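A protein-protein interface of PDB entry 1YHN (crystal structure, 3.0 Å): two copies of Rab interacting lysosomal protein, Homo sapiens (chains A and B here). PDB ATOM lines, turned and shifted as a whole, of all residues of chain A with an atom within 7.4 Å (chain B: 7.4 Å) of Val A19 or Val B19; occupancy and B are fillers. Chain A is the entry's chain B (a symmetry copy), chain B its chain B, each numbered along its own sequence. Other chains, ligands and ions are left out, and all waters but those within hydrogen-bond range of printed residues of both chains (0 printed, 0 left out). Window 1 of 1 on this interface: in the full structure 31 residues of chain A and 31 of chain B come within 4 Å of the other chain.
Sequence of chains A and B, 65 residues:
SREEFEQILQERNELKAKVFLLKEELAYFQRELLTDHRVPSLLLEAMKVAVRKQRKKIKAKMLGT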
ATOM      1  N   ARG A  12      14.614  -2.071 -28.655  1.00  0.00           N
ATOM      2  CA  ARG A  12      13.665  -3.140 -28.913  1.00  0.00           C
ATOM      3  C   ARG A  12      14.453  -4.403 -29.236  1.00  0.00           C
ATOM      4  O   ARG A  12      14.136  -5.482 -28.752  1.00  0.00           O
ATOM      5  CB  ARG A  12      12.746  -2.767 -30.082  1.00  0.00           C
ATOM      6  CG  ARG A  12      11.409  -3.496 -30.073  1.00  0.00           C
ATOM      7  CD  ARG A  12      11.440  -4.826 -30.815  1.00  0.00           C
ATOM      8  NE  ARG A  12      11.336  -4.643 -32.264  1.00  0.00           N
ATOM      9  CZ  ARG A  12      12.371  -4.399 -33.060  1.00  0.00           C
ATOM     10  NH1 ARG A  12      13.588  -4.318 -32.546  1.00  0.00           N
ATOM     11  NH2 ARG A  12      12.192  -4.227 -34.360  1.00  0.00           N
ATOM     12  N   ASN A  13      15.498  -4.259 -30.043  1.00  0.00           N
ATOM     13  CA  ASN A  13      16.318  -5.400 -30.423  1.00  0.00           C
ATOM     14  C   ASN A  13      17.026  -5.979 -29.216  1.00  0.00           C
ATOM     15  O   ASN A  13      16.933  -7.181 -28.929  1.00  0.00           O
ATOM     16  CB  ASN A  13      17.366  -5.005 -31.465  1.00  0.00           C
ATOM     17  CG  ASN A  13      16.759  -4.708 -32.817  1.00  0.00           C
ATOM     18  OD1 ASN A  13      15.748  -5.299 -33.190  1.00  0.00           O
ATOM     19  ND2 ASN A  13      17.385  -3.803 -33.570  1.00  0.00           N
ATOM     20  N   GLU A  14      17.738  -5.116 -28.509  1.00  0.00           N
ATOM     21  CA  GLU A  14      18.469  -5.543 -27.337  1.00  0.00           C
ATOM     22  C   GLU A  14      17.585  -6.332 -26.400  1.00  0.00           C
ATOM     23  O   GLU A  14      17.921  -7.438 -26.011  1.00  0.00           O
ATOM     24  CB  GLU A  14      19.030  -4.347 -26.619  1.00  0.00           C
ATOM     25  CG  GLU A  14      20.064  -4.742 -25.635  1.00  0.00           C
ATOM     26  CD  GLU A  14      21.046  -3.638 -25.397  1.00  0.00           C
ATOM     27  OE1 GLU A  14      22.080  -3.918 -24.750  1.00  0.00           O
ATOM     28  OE2 GLU A  14      20.782  -2.497 -25.861  1.00  0.00           O
ATOM     29  N   LEU A  15      16.446  -5.768 -26.037  1.00  0.00           N
ATOM     30  CA  LEU A  15      15.531  -6.469 -25.160  1.00  0.00           C
ATOM     31  C   LEU A  15      14.986  -7.774 -25.754  1.00  0.00           C
ATOM     32  O   LEU A  15      14.868  -8.777 -25.050  1.00  0.00           O
ATOM     33  CB  LEU A  15      14.389  -5.538 -24.756  1.00  0.00           C
ATOM     34  CG  LEU A  15      14.909  -4.519 -23.740  1.00  0.00           C
ATOM     35  CD1 LEU A  15      13.807  -3.574 -23.319  1.00  0.00           C
ATOM     36  CD2 LEU A  15      15.461  -5.269 -22.534  1.00  0.00           C
ATOM     37  N   LYS A  16      14.660  -7.776 -27.043  1.00  0.00           N
ATOM     38  CA  LYS A  16      14.154  -8.994 -27.648  1.00  0.00           C
ATOM     39  C   LYS A  16      15.218 -10.051 -27.442  1.00  0.00           C
ATOM     40  O   LYS A  16      14.918 -11.180 -27.056  1.00  0.00           O
ATOM     41  CB  LYS A  16      13.872  -8.810 -29.145  1.00  0.00           C
ATOM     42  CG  LYS A  16      13.485 -10.118 -29.852  1.00  0.00           C
ATOM     43  CD  LYS A  16      12.845  -9.928 -31.232  1.00  0.00           C
ATOM     44  CE  LYS A  16      11.368  -9.564 -31.116  1.00  0.00           C
ATOM     45  NZ  LYS A  16      10.708  -9.284 -32.425  1.00  0.00           N
ATOM     46  N   ALA A  17      16.468  -9.674 -27.679  1.00  0.00           N
ATOM     47  CA  ALA A  17      17.578 -10.598 -27.521  1.00  0.00           C
ATOM     48  C   ALA A  17      17.683 -11.127 -26.094  1.00  0.00           C
ATOM     49  O   ALA A  17      17.786 -12.332 -25.875  1.00  0.00           O
ATOM     50  CB  ALA A  17      18.851  -9.917 -27.910  1.00  0.00           C
ATOM     51  N   LYS A  18      17.666 -10.219 -25.123  1.00  0.00           N
ATOM     52  CA  LYS A  18      17.744 -10.601 -23.718  1.00  0.00           C
ATOM     53  C   LYS A  18      16.661 -11.622 -23.439  1.00  0.00           C
ATOM     54  O   LYS A  18      16.943 -12.723 -22.956  1.00  0.00           O
ATOM     55  CB  LYS A  18      17.543  -9.381 -22.813  1.00  0.00           C
ATOM     56  CG  LYS A  18      18.710  -8.393 -22.756  1.00  0.00           C
ATOM     57  CD  LYS A  18      18.282  -7.088 -22.069  1.00  0.00           C
ATOM     58  CE  LYS A  18      19.452  -6.184 -21.642  1.00  0.00           C
ATOM     59  NZ  LYS A  18      20.248  -5.593 -22.761  1.00  0.00           N
ATOM     60  N   VAL A  19      15.421 -11.265 -23.765  1.00  0.00           N
ATOM     61  CA  VAL A  19      14.299 -12.170 -23.534  1.00  0.00           C
ATOM     62  C   VAL A  19      14.548 -13.559 -24.109  1.00  0.00           C
ATOM     63  O   VAL A  19      14.064 -14.546 -23.583  1.00  0.00           O
ATOM     64  CB  VAL A  19      12.983 -11.612 -24.104  1.00  0.00           C
ATOM     65  CG1 VAL A  19      11.836 -12.489 -23.696  1.00  0.00           C
ATOM     66  CG2 VAL A  19      12.756 -10.207 -23.583  1.00  0.00           C
ATOM     67  N   PHE A  20      15.306 -13.650 -25.187  1.00  0.00           N
ATOM     68  CA  PHE A  20      15.592 -14.964 -25.743  1.00  0.00           C
ATOM     69  C   PHE A  20      16.555 -15.706 -24.821  1.00  0.00           C
ATOM     70  O   PHE A  20      16.323 -16.864 -24.470  1.00  0.00           O
ATOM     71  CB  PHE A  20      16.231 -14.843 -27.127  1.00  0.00           C
ATOM     72  CG  PHE A  20      16.788 -16.137 -27.646  1.00  0.00           C
ATOM     73  CD1 PHE A  20      15.943 -17.142 -28.093  1.00  0.00           C
ATOM     74  CD2 PHE A  20      18.152 -16.372 -27.636  1.00  0.00           C
ATOM     75  CE1 PHE A  20      16.453 -18.358 -28.516  1.00  0.00           C
ATOM     76  CE2 PHE A  20      18.662 -17.586 -28.058  1.00  0.00           C
ATOM     77  CZ  PHE A  20      17.814 -18.578 -28.497  1.00  0.00           C
ATOM     78  N   LEU A  21      17.637 -15.021 -24.446  1.00  0.00           N
ATOM     79  CA  LEU A  21      18.678 -15.574 -23.591  1.00  0.00           C
ATOM     80  C   LEU A  21      18.172 -15.941 -22.218  1.00  0.00           C
ATOM     81  O   LEU A  21      18.433 -17.031 -21.721  1.00  0.00           O
ATOM     82  CB  LEU A  21      19.827 -14.579 -23.461  1.00  0.00           C
ATOM     83  CG  LEU A  21      20.442 -14.167 -24.803  1.00  0.00           C
ATOM     84  CD1 LEU A  21      21.595 -13.195 -24.587  1.00  0.00           C
ATOM     85  CD2 LEU A  21      20.915 -15.409 -25.533  1.00  0.00           C
ATOM     86  N   LEU A  22      17.454 -15.034 -21.582  1.00  0.00           N
ATOM     87  CA  LEU A  22      16.926 -15.347 -20.271  1.00  0.00           C
ATOM     88  C   LEU A  22      16.101 -16.624 -20.378  1.00  0.00           C
ATOM     89  O   LEU A  22      16.142 -17.467 -19.498  1.00  0.00           O
ATOM     90  CB  LEU A  22      16.077 -14.192 -19.760  1.00  0.00           C
ATOM     91  CG  LEU A  22      16.864 -12.896 -19.566  1.00  0.00           C
ATOM     92  CD1 LEU A  22      15.952 -11.834 -18.989  1.00  0.00           C
ATOM     93  CD2 LEU A  22      18.043 -13.140 -18.642  1.00  0.00           C
ATOM     94  N   LYS A  23      15.353 -16.768 -21.465  1.00  0.00           N
ATOM     95  CA  LYS A  23      14.556 -17.969 -21.686  1.00  0.00           C
ATOM     96  C   LYS A  23      15.461 -19.192 -21.640  1.00  0.00           C
ATOM     97  O   LYS A  23      15.073 -20.234 -21.124  1.00  0.00           O
ATOM     98  CB  LYS A  23      13.851 -17.924 -23.048  1.00  0.00           C
ATOM     99  CG  LYS A  23      12.646 -17.012 -23.115  1.00  0.00           C
ATOM    100  CD  LYS A  23      11.576 -17.439 -22.144  1.00  0.00           C
ATOM    101  CE  LYS A  23      10.320 -16.587 -22.306  1.00  0.00           C
ATOM    102  NZ  LYS A  23       9.613 -16.849 -23.587  1.00  0.00           N
ATOM    103  N   GLU A  24      16.660 -19.073 -22.196  1.00  0.00           N
ATOM    104  CA  GLU A  24      17.599 -20.183 -22.171  1.00  0.00           C
ATOM    105  C   GLU A  24      17.965 -20.438 -20.717  1.00  0.00           C
ATOM    106  O   GLU A  24      17.578 -21.443 -20.128  1.00  0.00           O
ATOM    107  CB  GLU A  24      18.870 -19.854 -22.963  1.00  0.00           C
ATOM    108  CG  GLU A  24      18.664 -19.733 -24.465  1.00  0.00           C
ATOM    109  CD  GLU A  24      17.846 -20.883 -25.051  1.00  0.00           C
ATOM    110  OE1 GLU A  24      16.696 -20.636 -25.488  1.00  0.00           O
ATOM    111  OE2 GLU A  24      18.346 -22.029 -25.073  1.00  0.00           O
ATOM    112  N   ARG A  55       3.271 -15.107 -13.531  1.00  0.00           N
ATOM    113  CA  ARG A  55       3.798 -14.212 -14.533  1.00  0.00           C
ATOM    114  C   ARG A  55       2.641 -13.445 -15.142  1.00  0.00           C
ATOM    115  O   ARG A  55       2.555 -12.235 -14.995  1.00  0.00           O
ATOM    116  CB  ARG A  55       4.535 -14.993 -15.620  1.00  0.00           C
ATOM    117  CG  ARG A  55       5.310 -14.083 -16.553  1.00  0.00           C
ATOM    118  CD  ARG A  55       5.787 -14.783 -17.811  1.00  0.00           C
ATOM    119  NE  ARG A  55       6.945 -15.637 -17.583  1.00  0.00           N
ATOM    120  CZ  ARG A  55       7.674 -16.173 -18.562  1.00  0.00           C
ATOM    121  NH1 ARG A  55       7.358 -15.936 -19.833  1.00  0.00           N
ATOM    122  NH2 ARG A  55       8.718 -16.949 -18.278  1.00  0.00           N
ATOM    123  N   MET A  62       1.607  -4.700 -14.957  1.00  0.00           N
ATOM    124  CA  MET A  62       2.773  -3.906 -15.290  1.00  0.00           C
ATOM    125  C   MET A  62       2.487  -3.092 -16.543  1.00  0.00           C
ATOM    126  O   MET A  62       2.812  -1.906 -16.616  1.00  0.00           O
ATOM    127  CB  MET A  62       3.999  -4.792 -15.541  1.00  0.00           C
ATOM    128  CG  MET A  62       4.613  -5.428 -14.297  1.00  0.00           C
ATOM    129  SD  MET A  62       6.398  -5.630 -14.496  1.00  0.00           S
ATOM    130  CE  MET A  62       6.414  -6.717 -15.842  1.00  0.00           C
ATOM    131  N   ARG B  12       8.676  -2.257 -27.020  1.00  0.00           N
ATOM    132  CA  ARG B  12       9.811  -1.945 -26.171  1.00  0.00           C
ATOM    133  C   ARG B  12       9.378  -2.121 -24.721  1.00  0.00           C
ATOM    134  O   ARG B  12      10.102  -2.692 -23.914  1.00  0.00           O
ATOM    135  CB  ARG B  12      10.283  -0.508 -26.419  1.00  0.00           C
ATOM    136  CG  ARG B  12      11.740  -0.264 -26.048  1.00  0.00           C
ATOM    137  CD  ARG B  12      11.933   0.162 -24.597  1.00  0.00           C
ATOM    138  NE  ARG B  12      11.640   1.583 -24.405  1.00  0.00           N
ATOM    139  CZ  ARG B  12      10.425   2.070 -24.180  1.00  0.00           C
ATOM    140  NH1 ARG B  12       9.391   1.246 -24.113  1.00  0.00           N
ATOM    141  NH2 ARG B  12      10.241   3.373 -24.034  1.00  0.00           N
ATOM    142  N   ASN B  13       8.180  -1.647 -24.398  1.00  0.00           N
ATOM    143  CA  ASN B  13       7.669  -1.756 -23.039  1.00  0.00           C
ATOM    144  C   ASN B  13       7.462  -3.207 -22.658  1.00  0.00           C
ATOM    145  O   ASN B  13       7.969  -3.683 -21.632  1.00  0.00           O
ATOM    146  CB  ASN B  13       6.340  -1.013 -22.888  1.00  0.00           C
ATOM    147  CG  ASN B  13       6.503   0.488 -22.943  1.00  0.00           C
ATOM    148  OD1 ASN B  13       7.529   1.020 -22.524  1.00  0.00           O
ATOM    149  ND2 ASN B  13       5.482   1.185 -23.443  1.00  0.00           N
ATOM    150  N   GLU B  14       6.710  -3.910 -23.491  1.00  0.00           N
ATOM    151  CA  GLU B  14       6.429  -5.304 -23.237  1.00  0.00           C
ATOM    152  C   GLU B  14       7.698  -6.075 -22.953  1.00  0.00           C
ATOM    153  O   GLU B  14       7.802  -6.754 -21.946  1.00  0.00           O
ATOM    154  CB  GLU B  14       5.721  -5.908 -24.418  1.00  0.00           C
ATOM    155  CG  GLU B  14       5.106  -7.211 -24.074  1.00  0.00           C
ATOM    156  CD  GLU B  14       3.925  -7.507 -24.944  1.00  0.00           C
ATOM    157  OE1 GLU B  14       3.198  -8.472 -24.616  1.00  0.00           O
ATOM    158  OE2 GLU B  14       3.727  -6.773 -25.947  1.00  0.00           O
ATOM    159  N   LEU B  15       8.671  -5.968 -23.841  1.00  0.00           N
ATOM    160  CA  LEU B  15       9.928  -6.656 -23.632  1.00  0.00           C
ATOM    161  C   LEU B  15      10.682  -6.193 -22.378  1.00  0.00           C
ATOM    162  O   LEU B  15      11.250  -7.013 -21.655  1.00  0.00           O
ATOM    163  CB  LEU B  15      10.806  -6.515 -24.875  1.00  0.00           C
ATOM    164  CG  LEU B  15      10.258  -7.420 -25.980  1.00  0.00           C
ATOM    165  CD1 LEU B  15      11.099  -7.304 -27.231  1.00  0.00           C
ATOM    166  CD2 LEU B  15      10.246  -8.857 -25.474  1.00  0.00           C
ATOM    167  N   LYS B  16      10.687  -4.892 -22.106  1.00  0.00           N
ATOM    168  CA  LYS B  16      11.375  -4.415 -20.921  1.00  0.00           C
ATOM    169  C   LYS B  16      10.749  -5.128 -19.742  1.00  0.00           C
ATOM    170  O   LYS B  16      11.449  -5.621 -18.859  1.00  0.00           O
ATOM    171  CB  LYS B  16      11.237  -2.896 -20.757  1.00  0.00           C
ATOM    172  CG  LYS B  16      11.819  -2.375 -19.433  1.00  0.00           C
ATOM    173  CD  LYS B  16      12.038  -0.859 -19.389  1.00  0.00           C
ATOM    174  CE  LYS B  16      13.327  -0.460 -20.101  1.00  0.00           C
ATOM    175  NZ  LYS B  16      13.554   1.013 -20.165  1.00  0.00           N
ATOM    176  N   ALA B  17       9.423  -5.201 -19.743  1.00  0.00           N
ATOM    177  CA  ALA B  17       8.703  -5.857 -18.664  1.00  0.00           C
ATOM    178  C   ALA B  17       9.092  -7.326 -18.528  1.00  0.00           C
ATOM    179  O   ALA B  17       9.402  -7.796 -17.436  1.00  0.00           O
ATOM    180  CB  ALA B  17       7.232  -5.736 -18.904  1.00  0.00           C
ATOM    181  N   LYS B  18       9.063  -8.051 -19.642  1.00  0.00           N
ATOM    182  CA  LYS B  18       9.428  -9.463 -19.643  1.00  0.00           C
ATOM    183  C   LYS B  18      10.797  -9.604 -19.012  1.00  0.00           C
ATOM    184  O   LYS B  18      10.973 -10.354 -18.047  1.00  0.00           O
ATOM    185  CB  LYS B  18       9.464 -10.013 -21.073  1.00  0.00           C
ATOM    186  CG  LYS B  18       8.103 -10.217 -21.743  1.00  0.00           C
ATOM    187  CD  LYS B  18       8.274 -10.478 -23.246  1.00  0.00           C
ATOM    188  CE  LYS B  18       7.021 -11.047 -23.936  1.00  0.00           C
ATOM    189  NZ  LYS B  18       5.851 -10.120 -24.006  1.00  0.00           N
ATOM    190  N   VAL B  19      11.767  -8.864 -19.545  1.00  0.00           N
ATOM    191  CA  VAL B  19      13.127  -8.926 -19.019  1.00  0.00           C
ATOM    192  C   VAL B  19      13.173  -8.733 -17.509  1.00  0.00           C
ATOM    193  O   VAL B  19      14.035  -9.275 -16.838  1.00  0.00           O
ATOM    194  CB  VAL B  19      14.052  -7.896 -19.692  1.00  0.00           C
ATOM    195  CG1 VAL B  19      15.468  -8.110 -19.246  1.00  0.00           C
ATOM    196  CG2 VAL B  19      13.968  -8.042 -21.199  1.00  0.00           C
ATOM    197  N   PHE B  20      12.249  -7.965 -16.959  1.00  0.00           N
ATOM    198  CA  PHE B  20      12.243  -7.787 -15.516  1.00  0.00           C
ATOM    199  C   PHE B  20      11.781  -9.078 -14.846  1.00  0.00           C
ATOM    200  O   PHE B  20      12.419  -9.564 -13.910  1.00  0.00           O
ATOM    201  CB  PHE B  20      11.295  -6.657 -15.111  1.00  0.00           C
ATOM    202  CG  PHE B  20      11.041  -6.587 -13.632  1.00  0.00           C
ATOM    203  CD1 PHE B  20      12.017  -6.117 -12.768  1.00  0.00           C
ATOM    204  CD2 PHE B  20       9.847  -7.046 -13.100  1.00  0.00           C
ATOM    205  CE1 PHE B  20      11.805  -6.109 -11.399  1.00  0.00           C
ATOM    206  CE2 PHE B  20       9.635  -7.038 -11.734  1.00  0.00           C
ATOM    207  CZ  PHE B  20      10.613  -6.571 -10.885  1.00  0.00           C
ATOM    208  N   LEU B  21      10.663  -9.614 -15.337  1.00  0.00           N
ATOM    209  CA  LEU B  21      10.058 -10.828 -14.809  1.00  0.00           C
ATOM    210  C   LEU B  21      10.952 -12.035 -14.951  1.00  0.00           C
ATOM    211  O   LEU B  21      11.146 -12.790 -14.004  1.00  0.00           O
ATOM    212  CB  LEU B  21       8.729 -11.095 -15.509  1.00  0.00           C
ATOM    213  CG  LEU B  21       7.727  -9.941 -15.393  1.00  0.00           C
ATOM    214  CD1 LEU B  21       6.422 -10.293 -16.094  1.00  0.00           C
ATOM    215  CD2 LEU B  21       7.487  -9.639 -13.927  1.00  0.00           C
ATOM    216  N   LEU B  22      11.497 -12.241 -16.136  1.00  0.00           N
ATOM    217  CA  LEU B  22      12.381 -13.373 -16.316  1.00  0.00           C
ATOM    218  C   LEU B  22      13.499 -13.279 -15.283  1.00  0.00           C
ATOM    219  O   LEU B  22      13.913 -14.279 -14.721  1.00  0.00           O
ATOM    220  CB  LEU B  22      12.946 -13.375 -17.729  1.00  0.00           C
ATOM    221  CG  LEU B  22      11.879 -13.536 -18.812  1.00  0.00           C
ATOM    222  CD1 LEU B  22      12.545 -13.599 -20.170  1.00  0.00           C
ATOM    223  CD2 LEU B  22      11.072 -14.796 -18.559  1.00  0.00           C
ATOM    224  N   LYS B  23      13.983 -12.070 -15.030  1.00  0.00           N
ATOM    225  CA  LYS B  23      15.026 -11.862 -14.030  1.00  0.00           C
ATOM    226  C   LYS B  23      14.558 -12.411 -12.690  1.00  0.00           C
ATOM    227  O   LYS B  23      15.344 -12.982 -11.944  1.00  0.00           O
ATOM    228  CB  LYS B  23      15.352 -10.372 -13.870  1.00  0.00           C
ATOM    229  CG  LYS B  23      16.185  -9.775 -14.984  1.00  0.00           C
ATOM    230  CD  LYS B  23      17.527 -10.451 -15.092  1.00  0.00           C
ATOM    231  CE  LYS B  23      18.403  -9.763 -16.135  1.00  0.00           C
ATOM    232  NZ  LYS B  23      18.840  -8.408 -15.710  1.00  0.00           N
ATOM    233  N   GLU B  24      13.283 -12.221 -12.376  1.00  0.00           N
ATOM    234  CA  GLU B  24      12.745 -12.738 -11.128  1.00  0.00           C
ATOM    235  C   GLU B  24      12.817 -14.256 -11.194  1.00  0.00           C
ATOM    236  O   GLU B  24      13.608 -14.888 -10.501  1.00  0.00           O
ATOM    237  CB  GLU B  24      11.287 -12.308 -10.930  1.00  0.00           C
ATOM    238  CG  GLU B  24      11.096 -10.819 -10.688  1.00  0.00           C
ATOM    239  CD  GLU B  24      12.058 -10.254  -9.644  1.00  0.00           C
ATOM    240  OE1 GLU B  24      12.950  -9.458 -10.023  1.00  0.00           O
ATOM    241  OE2 GLU B  24      11.927 -10.604  -8.451  1.00  0.00           O
ATOM    242  N   ARG B  55      26.528 -15.604 -21.498  1.00  0.00           N
ATOM    243  CA  ARG B  55      25.544 -14.647 -21.945  1.00  0.00           C
ATOM    244  C   ARG B  55      26.250 -13.586 -22.766  1.00  0.00           C
ATOM    245  O   ARG B  55      26.007 -13.462 -23.957  1.00  0.00           O
ATOM    246  CB  ARG B  55      24.840 -13.999 -20.753  1.00  0.00           C
ATOM    247  CG  ARG B  55      23.638 -13.179 -21.175  1.00  0.00           C
ATOM    248  CD  ARG B  55      23.111 -12.279 -20.073  1.00  0.00           C
ATOM    249  NE  ARG B  55      22.343 -13.001 -19.068  1.00  0.00           N
ATOM    250  CZ  ARG B  55      21.599 -12.405 -18.136  1.00  0.00           C
ATOM    251  NH1 ARG B  55      21.528 -11.076 -18.090  1.00  0.00           N
ATOM    252  NH2 ARG B  55      20.924 -13.129 -17.246  1.00  0.00           N
ATOM    253  N   MET B  62      24.673 -11.747 -31.234  1.00  0.00           N
ATOM    254  CA  MET B  62      23.280 -11.624 -31.619  1.00  0.00           C
ATOM    255  C   MET B  62      23.017 -10.210 -32.110  1.00  0.00           C
ATOM    256  O   MET B  62      22.348 -10.006 -33.125  1.00  0.00           O
ATOM    257  CB  MET B  62      22.347 -11.924 -30.440  1.00  0.00           C
ATOM    258  CG  MET B  62      22.253 -13.394 -30.036  1.00  0.00           C
ATOM    259  SD  MET B  62      20.610 -13.773 -29.382  1.00  0.00           S
ATOM    260  CE  MET B  62      20.606 -12.731 -28.001  1.00  0.00           C
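Among the printed residues, pairs that only touch across the chains: Leu A22 with Arg B55, Arg A55 with Leu B22, Ala A17 with Met B62, Met A62 with Ala B17, Val A19 with Leu B15, Leu A15 with Val B19, Val A19 with Val B19, Leu A21 with Met B62, Met A62 with Leu B21, Lys A16 with Leu B15, Leu A15 with Lys B16, Leu A22 with Leu B22, Leu A15 with Leu B15, Val A19 with Leu B22, Leu A22 with Val B19, Arg A12 with Leu B15, Leu A15 with Arg B12, Arg A55 with Leu B21, Leu A21 with Arg B55, Phe A20 with Met B62 and Met A62 with Phe B20.
Val A19 touches just these residues of chain B: Leu B15, Val B19 and Leu B22. Val B19 touches three residues of chain A. Of the printed residues of chain A, Phe B20 touches Met A62 (3.98 Å). Of the printed residues of chain A, Leu B21 touches Arg A55 and Met A62. Printed residues of chain A within 4 Å of Arg B55: Leu A21 (3.98 Å) and Leu A22 (3.2 Å). The nearest residue of chain B that does not touch Val A19 is Lys B18 (4.1 Å). The nearest residue of chain A that does not touch Val B19 is Lys A18 (4.1 Å).
Arg A12 touches Leu B15, and with the chains exchanged Leu A15 touches Arg B12. Val A19 touches Leu B22, and with the chains exchanged Leu A22 touches Val B19. Phe A20 touches Met B62, and with the chains exchanged Met A62 touches Phe B20. Leu A22 touches its own counterpart, Leu B22. Positions printed for both chains: 12, 13, 14, 15, 16, 17, 18, 19, 20, 21, 22, 23, 24, 55 and 62. Of the 21 pairs that touch across the chains among the printed residues, 21 have their exchanged pair printed and touching as well.
Of the 15 printed residues of chain B, 10 touch a printed residue of chain A. Hydrophobic or aromatic side chains of chain B that line the printed part of chain A: Leu B15, Ala B17, Val B19, Phe B20, Leu B21, Leu B22 and Met B62. Printed residues of chain A that touch a printed residue of chain B: Arg A12, Leu A15, Lys A16, Ala A17, Val A19, Phe A20, Leu A21, Leu A22, Arg A55 and Met A62. Among the printed residues, 21 pairs touch across the chains.
The guanidinium group (NH1) of Arg A12 is in hydrogen-bond range of the side-chain amide oxygen (OD1) of Asn A13. The side-chain amide oxygen of Asn B13 is in hydrogen-bond range of the guanidinium group of Arg B12 (2.5 Å).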
